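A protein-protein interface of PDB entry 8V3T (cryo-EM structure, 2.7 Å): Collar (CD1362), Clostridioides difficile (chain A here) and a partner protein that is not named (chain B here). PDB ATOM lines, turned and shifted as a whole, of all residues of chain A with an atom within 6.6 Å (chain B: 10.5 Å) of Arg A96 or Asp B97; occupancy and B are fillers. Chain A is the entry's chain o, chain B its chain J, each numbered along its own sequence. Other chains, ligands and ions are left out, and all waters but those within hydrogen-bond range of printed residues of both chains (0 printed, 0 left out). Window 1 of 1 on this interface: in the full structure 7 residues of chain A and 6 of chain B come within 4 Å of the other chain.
N of Arg B7 is in hydrogen-bond range of O of Asp B97. The side-chain amide nitrogen (ND2) of Asn B8 lies within hydrogen-bond range of the side-chain carboxylate (OD2) of Asp B97 (2.8 Å). The backbone NH (N) of Asp B97 sits at hydrogen-bond distance from the side-chain carboxylate (OD1) of Asp B95, at 3.0 Å. The side-chain carboxylate (OD2) of Asp A126 is in hydrogen-bond range of the backbone NH (N) of Leu A2, at 2.9 Å. The backbone carbonyl oxygen (O) of Leu A125 sits at hydrogen-bond distance from the guanidinium group (NH1) of Arg A96 (2.9 Å). The backbone carbonyl oxygen (O) of Asn A99 sits at hydrogen-bond distance from the backbone NH (N) of Asn A123.
Printed residues of chain B that touch a printed residue of chain A: Arg B7, Asn B8, Val B9, Trp B14, Pro B96 and Asp B97. Along chain B the printed residues that touch a printed residue of chain A span positions 7 to 97. Hydrophobic or aromatic side chains of chain A within 4 Å of the printed part of chain B: Tyr A124 and Leu A125.
The side-chain carboxylate (OD1) of Asp A126 lies within salt-bridge range of the guanidinium group (NE) of Arg B7. The guanidinium group (NH2) of Arg A96 lies within hydrogen-bond range of the side-chain amide oxygen (OD1) of Asn B8. The backbone NH (N) of Leu A125 sits at hydrogen-bond distance from the side-chain amide oxygen (OD1) of Asn B8, 2.8 Å away. The guanidinium group of Arg A96 is in salt-bridge range of the side-chain carboxylate of Asp B97 (2.8 Å). The guanidinium group (NE) of Arg B7 lies close to the guanidinium group (NH1) of Arg A96 (3.0 Å). O of Lys A97 lies close to OD2 of Asp B97 (2.8 Å).
No residue of chain B comes within 4 Å of Lys A92. Val A93 touches none of the printed residues of chain B. Arg A96 touches just these residues of chain B: Arg B7 (3.0 Å), Asn B8 (3.0 Å) and Asp B97 (2.8 Å). Lys A97 touches two residues of chain B. Of chain B, only Asn B8 (3.6 Å) comes within 4 Å of Tyr A124. Printed residues of chain A within 4 Å of Val B9: Leu A125. Of the printed residues of chain A, Trp B14 touches Asn A90 (3.5 Å) and Asn A99 (3.5 Å). Of chain A, only Arg A96 (2.8 Å) and Lys A97 (2.8 Å) come within 4 Å of Asp B97. Ile B142 touches none of the printed residues of chain A. The nearest residue of chain B that does not touch Arg A96 is Val B9 (6.6 Å).
Among the printed residues, pairs that only touch across the chains: Asn A90 with Trp B14, Lys A97 with Pro B96, Asn A99 with Trp B14, Tyr A124 with Asn B8, Leu A125 with Arg B7 and Leu A125 with Val B9.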
ATOM      1  N   LEU A   2     -13.786  20.380 -15.684  1.00  0.00           N
ATOM      2  CA  LEU A   2     -15.182  20.732 -15.905  1.00  0.00           C
ATOM      3  C   LEU A   2     -15.604  21.873 -14.985  1.00  0.00           C
ATOM      4  O   LEU A   2     -15.166  21.963 -13.836  1.00  0.00           O
ATOM      5  CB  LEU A   2     -16.070  19.510 -15.680  1.00  0.00           C
ATOM      6  CG  LEU A   2     -17.413  19.482 -16.408  1.00  0.00           C
ATOM      7  CD1 LEU A   2     -17.228  19.049 -17.848  1.00  0.00           C
ATOM      8  CD2 LEU A   2     -18.364  18.546 -15.697  1.00  0.00           C
ATOM      9  N   ASN A  90     -27.171   8.963 -16.358  1.00  0.00           N
ATOM     10  CA  ASN A  90     -26.108   9.931 -16.571  1.00  0.00           C
ATOM     11  C   ASN A  90     -26.679  11.136 -17.298  1.00  0.00           C
ATOM     12  O   ASN A  90     -27.740  11.065 -17.922  1.00  0.00           O
ATOM     13  CB  ASN A  90     -24.934   9.321 -17.349  1.00  0.00           C
ATOM     14  CG  ASN A  90     -25.360   8.671 -18.654  1.00  0.00           C
ATOM     15  OD1 ASN A  90     -26.146   9.229 -19.418  1.00  0.00           O
ATOM     16  ND2 ASN A  90     -24.834   7.483 -18.916  1.00  0.00           N
ATOM     17  N   ILE A  91     -25.961  12.248 -17.198  1.00  0.00           N
ATOM     18  CA  ILE A  91     -26.288  13.461 -17.932  1.00  0.00           C
ATOM     19  C   ILE A  91     -25.048  13.882 -18.703  1.00  0.00           C
ATOM     20  O   ILE A  91     -23.915  13.621 -18.284  1.00  0.00           O
ATOM     21  CB  ILE A  91     -26.779  14.598 -17.008  1.00  0.00           C
ATOM     22  CG1 ILE A  91     -25.674  15.044 -16.054  1.00  0.00           C
ATOM     23  CG2 ILE A  91     -27.997  14.158 -16.220  1.00  0.00           C
ATOM     24  CD1 ILE A  91     -26.087  16.181 -15.153  1.00  0.00           C
ATOM     25  N   LYS A  92     -25.262  14.520 -19.846  1.00  0.00           N
ATOM     26  CA  LYS A  92     -24.165  14.887 -20.728  1.00  0.00           C
ATOM     27  C   LYS A  92     -23.859  16.373 -20.593  1.00  0.00           C
ATOM     28  O   LYS A  92     -24.722  17.217 -20.854  1.00  0.00           O
ATOM     29  CB  LYS A  92     -24.486  14.538 -22.181  1.00  0.00           C
ATOM     30  CG  LYS A  92     -23.298  14.722 -23.105  1.00  0.00           C
ATOM     31  CD  LYS A  92     -23.648  14.434 -24.548  1.00  0.00           C
ATOM     32  CE  LYS A  92     -22.410  14.517 -25.423  1.00  0.00           C
ATOM     33  NZ  LYS A  92     -22.722  14.311 -26.862  1.00  0.00           N
ATOM     34  N   VAL A  93     -22.627  16.682 -20.193  1.00  0.00           N
ATOM     35  CA  VAL A  93     -22.167  18.052 -19.997  1.00  0.00           C
ATOM     36  C   VAL A  93     -20.849  18.215 -20.740  1.00  0.00           C
ATOM     37  O   VAL A  93     -19.855  17.571 -20.385  1.00  0.00           O
ATOM     38  CB  VAL A  93     -21.983  18.388 -18.507  1.00  0.00           C
ATOM     39  CG1 VAL A  93     -21.353  19.765 -18.345  1.00  0.00           C
ATOM     40  CG2 VAL A  93     -23.305  18.301 -17.769  1.00  0.00           C
ATOM     41  N   THR A  94     -20.837  19.084 -21.750  1.00  0.00           N
ATOM     42  CA  THR A  94     -19.639  19.432 -22.516  1.00  0.00           C
ATOM     43  C   THR A  94     -18.925  18.155 -22.982  1.00  0.00           C
ATOM     44  O   THR A  94     -17.900  17.727 -22.449  1.00  0.00           O
ATOM     45  CB  THR A  94     -18.737  20.367 -21.693  1.00  0.00           C
ATOM     46  OG1 THR A  94     -19.303  21.680 -21.702  1.00  0.00           O
ATOM     47  CG2 THR A  94     -17.349  20.514 -22.318  1.00  0.00           C
ATOM     48  N   ASP A  95     -19.575  17.501 -23.950  1.00  0.00           N
ATOM     49  CA  ASP A  95     -19.149  16.218 -24.507  1.00  0.00           C
ATOM     50  C   ASP A  95     -18.635  15.226 -23.461  1.00  0.00           C
ATOM     51  O   ASP A  95     -17.691  14.478 -23.728  1.00  0.00           O
ATOM     52  CB  ASP A  95     -18.118  16.435 -25.627  1.00  0.00           C
ATOM     53  CG  ASP A  95     -16.874  17.183 -25.170  1.00  0.00           C
ATOM     54  OD1 ASP A  95     -16.150  16.678 -24.288  1.00  0.00           O
ATOM     55  OD2 ASP A  95     -16.615  18.275 -25.713  1.00  0.00           O
ATOM     56  N   ARG A  96     -19.259  15.194 -22.280  1.00  0.00           N
ATOM     57  CA  ARG A  96     -18.942  14.201 -21.256  1.00  0.00           C
ATOM     58  C   ARG A  96     -20.220  13.735 -20.579  1.00  0.00           C
ATOM     59  O   ARG A  96     -21.133  14.532 -20.338  1.00  0.00           O
ATOM     60  CB  ARG A  96     -18.004  14.718 -20.168  1.00  0.00           C
ATOM     61  CG  ARG A  96     -17.366  13.584 -19.399  1.00  0.00           C
ATOM     62  CD  ARG A  96     -16.449  14.063 -18.301  1.00  0.00           C
ATOM     63  NE  ARG A  96     -16.091  12.943 -17.440  1.00  0.00           N
ATOM     64  CZ  ARG A  96     -15.362  13.021 -16.337  1.00  0.00           C
ATOM     65  NH1 ARG A  96     -14.947  14.180 -15.859  1.00  0.00           N
ATOM     66  NH2 ARG A  96     -15.017  11.900 -15.711  1.00  0.00           N
ATOM     67  N   LYS A  97     -20.267  12.444 -20.258  1.00  0.00           N
ATOM     68  CA  LYS A  97     -21.389  11.832 -19.559  1.00  0.00           C
ATOM     69  C   LYS A  97     -21.006  11.525 -18.116  1.00  0.00           C
ATOM     70  O   LYS A  97     -20.045  10.793 -17.866  1.00  0.00           O
ATOM     71  CB  LYS A  97     -21.838  10.563 -20.287  1.00  0.00           C
ATOM     72  CG  LYS A  97     -22.698  10.806 -21.520  1.00  0.00           C
ATOM     73  CD  LYS A  97     -22.549   9.689 -22.538  1.00  0.00           C
ATOM     74  CE  LYS A  97     -21.451  10.012 -23.558  1.00  0.00           C
ATOM     75  NZ  LYS A  97     -21.476   9.041 -24.693  1.00  0.00           N
ATOM     76  N   LEU A  98     -21.780  12.051 -17.170  1.00  0.00           N
ATOM     77  CA  LEU A  98     -21.469  11.937 -15.751  1.00  0.00           C
ATOM     78  C   LEU A  98     -22.458  10.994 -15.081  1.00  0.00           C
ATOM     79  O   LEU A  98     -23.670  11.218 -15.142  1.00  0.00           O
ATOM     80  CB  LEU A  98     -21.513  13.305 -15.066  1.00  0.00           C
ATOM     81  CG  LEU A  98     -20.830  14.477 -15.766  1.00  0.00           C
ATOM     82  CD1 LEU A  98     -20.997  15.737 -14.954  1.00  0.00           C
ATOM     83  CD2 LEU A  98     -19.378  14.191 -15.991  1.00  0.00           C
ATOM     84  N   ASN A  99     -21.944   9.965 -14.411  1.00  0.00           N
ATOM     85  CA  ASN A  99     -22.809   8.948 -13.826  1.00  0.00           C
ATOM     86  C   ASN A  99     -23.589   9.506 -12.638  1.00  0.00           C
ATOM     87  O   ASN A  99     -23.105  10.361 -11.895  1.00  0.00           O
ATOM     88  CB  ASN A  99     -21.989   7.737 -13.380  1.00  0.00           C
ATOM     89  CG  ASN A  99     -21.343   7.007 -14.540  1.00  0.00           C
ATOM     90  OD1 ASN A  99     -21.976   6.762 -15.567  1.00  0.00           O
ATOM     91  ND2 ASN A  99     -20.070   6.669 -14.387  1.00  0.00           N
ATOM     92  N   ASN A 123     -20.892  11.593  -9.717  1.00  0.00           N
ATOM     93  CA  ASN A 123     -19.554  11.110  -9.409  1.00  0.00           C
ATOM     94  C   ASN A 123     -18.726  11.072 -10.681  1.00  0.00           C
ATOM     95  O   ASN A 123     -19.172  10.529 -11.697  1.00  0.00           O
ATOM     96  CB  ASN A 123     -19.606   9.720  -8.775  1.00  0.00           C
ATOM     97  CG  ASN A 123     -18.319   9.352  -8.074  1.00  0.00           C
ATOM     98  OD1 ASN A 123     -18.095   9.728  -6.925  1.00  0.00           O
ATOM     99  ND2 ASN A 123     -17.464   8.610  -8.763  1.00  0.00           N
ATOM    100  N   TYR A 124     -17.521  11.633 -10.625  1.00  0.00           N
ATOM    101  CA  TYR A 124     -16.639  11.640 -11.784  1.00  0.00           C
ATOM    102  C   TYR A 124     -15.221  11.949 -11.327  1.00  0.00           C
ATOM    103  O   TYR A 124     -14.987  12.357 -10.188  1.00  0.00           O
ATOM    104  CB  TYR A 124     -17.123  12.638 -12.844  1.00  0.00           C
ATOM    105  CG  TYR A 124     -17.015  14.096 -12.457  1.00  0.00           C
ATOM    106  CD1 TYR A 124     -18.029  14.727 -11.749  1.00  0.00           C
ATOM    107  CD2 TYR A 124     -15.915  14.853 -12.833  1.00  0.00           C
ATOM    108  CE1 TYR A 124     -17.935  16.062 -11.405  1.00  0.00           C
ATOM    109  CE2 TYR A 124     -15.813  16.184 -12.494  1.00  0.00           C
ATOM    110  CZ  TYR A 124     -16.824  16.784 -11.781  1.00  0.00           C
ATOM    111  OH  TYR A 124     -16.719  18.114 -11.446  1.00  0.00           O
ATOM    112  N   LEU A 125     -14.275  11.740 -12.237  1.00  0.00           N
ATOM    113  CA  LEU A 125     -12.867  12.022 -12.004  1.00  0.00           C
ATOM    114  C   LEU A 125     -12.441  13.201 -12.865  1.00  0.00           C
ATOM    115  O   LEU A 125     -12.822  13.294 -14.035  1.00  0.00           O
ATOM    116  CB  LEU A 125     -11.993  10.809 -12.330  1.00  0.00           C
ATOM    117  CG  LEU A 125     -12.041   9.583 -11.417  1.00  0.00           C
ATOM    118  CD1 LEU A 125     -10.828   8.706 -11.664  1.00  0.00           C
ATOM    119  CD2 LEU A 125     -12.120   9.983  -9.961  1.00  0.00           C
ATOM    120  N   ASP A 126     -11.653  14.102 -12.287  1.00  0.00           N
ATOM    121  CA  ASP A 126     -11.155  15.255 -13.017  1.00  0.00           C
ATOM    122  C   ASP A 126      -9.672  15.440 -12.730  1.00  0.00           C
ATOM    123  O   ASP A 126      -9.154  14.991 -11.704  1.00  0.00           O
ATOM    124  CB  ASP A 126     -11.939  16.523 -12.660  1.00  0.00           C
ATOM    125  CG  ASP A 126     -12.374  17.296 -13.889  1.00  0.00           C
ATOM    126  OD1 ASP A 126     -12.260  16.749 -15.004  1.00  0.00           O
ATOM    127  OD2 ASP A 126     -12.849  18.440 -13.742  1.00  0.00           O
ATOM    128  N   ARG B   7     -12.937   9.607 -19.497  1.00  0.00           N
ATOM    129  CA  ARG B   7     -11.774   9.859 -18.655  1.00  0.00           C
ATOM    130  C   ARG B   7     -12.024   9.356 -17.230  1.00  0.00           C
ATOM    131  O   ARG B   7     -11.358   9.783 -16.292  1.00  0.00           O
ATOM    132  CB  ARG B   7     -11.435  11.338 -18.663  1.00  0.00           C
ATOM    133  CG  ARG B   7     -12.591  12.205 -18.218  1.00  0.00           C
ATOM    134  CD  ARG B   7     -12.097  13.583 -17.790  1.00  0.00           C
ATOM    135  NE  ARG B   7     -13.035  14.657 -18.091  1.00  0.00           N
ATOM    136  CZ  ARG B   7     -13.201  15.229 -19.276  1.00  0.00           C
ATOM    137  NH1 ARG B   7     -12.454  14.905 -20.313  1.00  0.00           N
ATOM    138  NH2 ARG B   7     -14.140  16.159 -19.423  1.00  0.00           N
ATOM    139  N   ASN B   8     -13.006   8.468 -17.077  1.00  0.00           N
ATOM    140  CA  ASN B   8     -13.300   7.832 -15.801  1.00  0.00           C
ATOM    141  C   ASN B   8     -12.756   6.411 -15.766  1.00  0.00           C
ATOM    142  O   ASN B   8     -12.442   5.813 -16.796  1.00  0.00           O
ATOM    143  CB  ASN B   8     -14.809   7.793 -15.534  1.00  0.00           C
ATOM    144  CG  ASN B   8     -15.282   8.951 -14.691  1.00  0.00           C
ATOM    145  OD1 ASN B   8     -14.511   9.511 -13.911  1.00  0.00           O
ATOM    146  ND2 ASN B   8     -16.560   9.283 -14.795  1.00  0.00           N
ATOM    147  N   VAL B   9     -12.636   5.881 -14.550  1.00  0.00           N
ATOM    148  CA  VAL B   9     -12.448   4.448 -14.380  1.00  0.00           C
ATOM    149  C   VAL B   9     -13.746   3.739 -14.754  1.00  0.00           C
ATOM    150  O   VAL B   9     -14.847   4.270 -14.558  1.00  0.00           O
ATOM    151  CB  VAL B   9     -12.032   4.125 -12.933  1.00  0.00           C
ATOM    152  CG1 VAL B   9     -11.419   2.743 -12.851  1.00  0.00           C
ATOM    153  CG2 VAL B   9     -11.056   5.168 -12.418  1.00  0.00           C
ATOM    154  N   MET B  10     -13.624   2.534 -15.313  1.00  0.00           N
ATOM    155  CA  MET B  10     -14.813   1.789 -15.707  1.00  0.00           C
ATOM    156  C   MET B  10     -15.643   1.430 -14.481  1.00  0.00           C
ATOM    157  O   MET B  10     -15.118   0.961 -13.467  1.00  0.00           O
ATOM    158  CB  MET B  10     -14.428   0.521 -16.469  1.00  0.00           C
ATOM    159  CG  MET B  10     -13.676   0.764 -17.764  1.00  0.00           C
ATOM    160  SD  MET B  10     -12.686  -0.662 -18.244  1.00  0.00           S
ATOM    161  CE  MET B  10     -11.227   0.156 -18.875  1.00  0.00           C
ATOM    162  N   SER B  11     -16.947   1.653 -14.580  1.00  0.00           N
ATOM    163  CA  SER B  11     -17.883   1.341 -13.513  1.00  0.00           C
ATOM    164  C   SER B  11     -18.600   0.038 -13.827  1.00  0.00           C
ATOM    165  O   SER B  11     -19.050  -0.180 -14.955  1.00  0.00           O
ATOM    166  CB  SER B  11     -18.898   2.469 -13.335  1.00  0.00           C
ATOM    167  OG  SER B  11     -19.688   2.263 -12.181  1.00  0.00           O
ATOM    168  N   TRP B  14     -22.127  -0.752 -15.757  1.00  0.00           N
ATOM    169  CA  TRP B  14     -22.224  -1.054 -17.185  1.00  0.00           C
ATOM    170  C   TRP B  14     -21.603  -2.406 -17.509  1.00  0.00           C
ATOM    171  O   TRP B  14     -20.699  -2.511 -18.334  1.00  0.00           O
ATOM    172  CB  TRP B  14     -21.570   0.056 -17.995  1.00  0.00           C
ATOM    173  CG  TRP B  14     -22.074   1.414 -17.636  1.00  0.00           C
ATOM    174  CD1 TRP B  14     -21.533   2.273 -16.728  1.00  0.00           C
ATOM    175  CD2 TRP B  14     -23.233   2.065 -18.165  1.00  0.00           C
ATOM    176  NE1 TRP B  14     -22.279   3.422 -16.662  1.00  0.00           N
ATOM    177  CE2 TRP B  14     -23.329   3.320 -17.534  1.00  0.00           C
ATOM    178  CE3 TRP B  14     -24.199   1.710 -19.110  1.00  0.00           C
ATOM    179  CZ2 TRP B  14     -24.349   4.221 -17.819  1.00  0.00           C
ATOM    180  CZ3 TRP B  14     -25.210   2.607 -19.391  1.00  0.00           C
ATOM    181  CH2 TRP B  14     -25.277   3.847 -18.749  1.00  0.00           C
ATOM    182  N   LEU B  93     -17.772  -4.991 -20.664  1.00  0.00           N
ATOM    183  CA  LEU B  93     -17.743  -3.821 -19.791  1.00  0.00           C
ATOM    184  C   LEU B  93     -17.560  -2.593 -20.671  1.00  0.00           C
ATOM    185  O   LEU B  93     -16.467  -2.357 -21.191  1.00  0.00           O
ATOM    186  CB  LEU B  93     -16.620  -3.935 -18.759  1.00  0.00           C
ATOM    187  CG  LEU B  93     -16.563  -2.899 -17.637  1.00  0.00           C
ATOM    188  CD1 LEU B  93     -17.812  -2.960 -16.779  1.00  0.00           C
ATOM    189  CD2 LEU B  93     -15.320  -3.114 -16.792  1.00  0.00           C
ATOM    190  N   ASN B  94     -18.630  -1.811 -20.841  1.00  0.00           N
ATOM    191  CA  ASN B  94     -18.626  -0.667 -21.759  1.00  0.00           C
ATOM    192  C   ASN B  94     -19.216   0.544 -21.037  1.00  0.00           C
ATOM    193  O   ASN B  94     -20.422   0.793 -21.096  1.00  0.00           O
ATOM    194  CB  ASN B  94     -19.396  -0.994 -23.033  1.00  0.00           C
ATOM    195  CG  ASN B  94     -19.262   0.083 -24.088  1.00  0.00           C
ATOM    196  OD1 ASN B  94     -18.283   0.825 -24.115  1.00  0.00           O
ATOM    197  ND2 ASN B  94     -20.252   0.173 -24.965  1.00  0.00           N
ATOM    198  N   ASP B  95     -18.354   1.294 -20.368  1.00  0.00           N
ATOM    199  CA  ASP B  95     -18.755   2.514 -19.678  1.00  0.00           C
ATOM    200  C   ASP B  95     -18.771   3.678 -20.665  1.00  0.00           C
ATOM    201  O   ASP B  95     -17.775   3.901 -21.360  1.00  0.00           O
ATOM    202  CB  ASP B  95     -17.795   2.797 -18.522  1.00  0.00           C
ATOM    203  CG  ASP B  95     -18.308   3.855 -17.559  1.00  0.00           C
ATOM    204  OD1 ASP B  95     -18.939   4.835 -17.999  1.00  0.00           O
ATOM    205  OD2 ASP B  95     -18.071   3.705 -16.344  1.00  0.00           O
ATOM    206  N   PRO B  96     -19.878   4.419 -20.771  1.00  0.00           N
ATOM    207  CA  PRO B  96     -19.913   5.542 -21.724  1.00  0.00           C
ATOM    208  C   PRO B  96     -18.849   6.595 -21.469  1.00  0.00           C
ATOM    209  O   PRO B  96     -18.345   7.201 -22.421  1.00  0.00           O
ATOM    210  CB  PRO B  96     -21.328   6.110 -21.541  1.00  0.00           C
ATOM    211  CG  PRO B  96     -22.116   4.994 -20.959  1.00  0.00           C
ATOM    212  CD  PRO B  96     -21.172   4.221 -20.101  1.00  0.00           C
ATOM    213  N   ASP B  97     -18.497   6.840 -20.207  1.00  0.00           N
ATOM    214  CA  ASP B  97     -17.477   7.831 -19.898  1.00  0.00           C
ATOM    215  C   ASP B  97     -16.061   7.289 -20.031  1.00  0.00           C
ATOM    216  O   ASP B  97     -15.115   8.081 -20.088  1.00  0.00           O
ATOM    217  CB  ASP B  97     -17.670   8.375 -18.483  1.00  0.00           C
ATOM    218  CG  ASP B  97     -17.286   9.834 -18.368  1.00  0.00           C
ATOM    219  OD1 ASP B  97     -16.954  10.438 -19.407  1.00  0.00           O
ATOM    220  OD2 ASP B  97     -17.304  10.375 -17.243  1.00  0.00           O
ATOM    221  N   SER B  98     -15.892   5.973 -20.079  1.00  0.00           N
ATOM    222  CA  SER B  98     -14.564   5.376 -20.105  1.00  0.00           C
ATOM    223  C   SER B  98     -13.983   5.468 -21.514  1.00  0.00           C
ATOM    224  O   SER B  98     -14.554   6.084 -22.417  1.00  0.00           O
ATOM    225  CB  SER B  98     -14.620   3.939 -19.598  1.00  0.00           C
ATOM    226  OG  SER B  98     -14.641   3.016 -20.671  1.00  0.00           O
ATOM    227  N   TYR B  99     -12.824   4.842 -21.711  1.00  0.00           N
ATOM    228  CA  TYR B  99     -12.101   4.974 -22.970  1.00  0.00           C
ATOM    229  C   TYR B  99     -12.633   4.022 -24.036  1.00  0.00           C
ATOM    230  O   TYR B  99     -12.709   4.391 -25.213  1.00  0.00           O
ATOM    231  CB  TYR B  99     -10.608   4.751 -22.730  1.00  0.00           C
ATOM    232  CG  TYR B  99     -10.014   5.704 -21.711  1.00  0.00           C
ATOM    233  CD1 TYR B  99     -10.156   5.478 -20.349  1.00  0.00           C
ATOM    234  CD2 TYR B  99      -9.315   6.834 -22.115  1.00  0.00           C
ATOM    235  CE1 TYR B  99      -9.623   6.349 -19.419  1.00  0.00           C
ATOM    236  CE2 TYR B  99      -8.774   7.708 -21.192  1.00  0.00           C
ATOM    237  CZ  TYR B  99      -8.931   7.459 -19.845  1.00  0.00           C
ATOM    238  OH  TYR B  99      -8.395   8.325 -18.922  1.00  0.00           O
ATOM    239  N   GLY B 100     -12.999   2.807 -23.654  1.00  0.00           N
ATOM    240  CA  GLY B 100     -13.503   1.860 -24.627  1.00  0.00           C
ATOM    241  C   GLY B 100     -14.168   0.679 -23.957  1.00  0.00           C
ATOM    242  O   GLY B 100     -14.318   0.634 -22.735  1.00  0.00           O
ATOM    243  N   ALA B 101     -14.569  -0.279 -24.783  1.00  0.00           N
ATOM    244  CA  ALA B 101     -15.218  -1.498 -24.326  1.00  0.00           C
ATOM    245  C   ALA B 101     -14.197  -2.618 -24.170  1.00  0.00           C
ATOM    246  O   ALA B 101     -13.101  -2.572 -24.732  1.00  0.00           O
ATOM    247  CB  ALA B 101     -16.321  -1.925 -25.296  1.00  0.00           C
ATOM    248  N   ILE B 142      -8.682  -2.978 -24.852  1.00  0.00           N
ATOM    249  CA  ILE B 142      -8.328  -1.568 -24.970  1.00  0.00           C
ATOM    250  C   ILE B 142      -6.817  -1.399 -25.067  1.00  0.00           C
ATOM    251  O   ILE B 142      -6.105  -1.496 -24.068  1.00  0.00           O
ATOM    252  CB  ILE B 142      -8.890  -0.757 -23.794  1.00  0.00           C
ATOM    253  CG1 ILE B 142     -10.405  -0.937 -23.705  1.00  0.00           C
ATOM    254  CG2 ILE B 142      -8.542   0.712 -23.946  1.00  0.00           C
ATOM    255  CD1 ILE B 142     -11.027  -0.258 -22.515  1.00  0.00           C
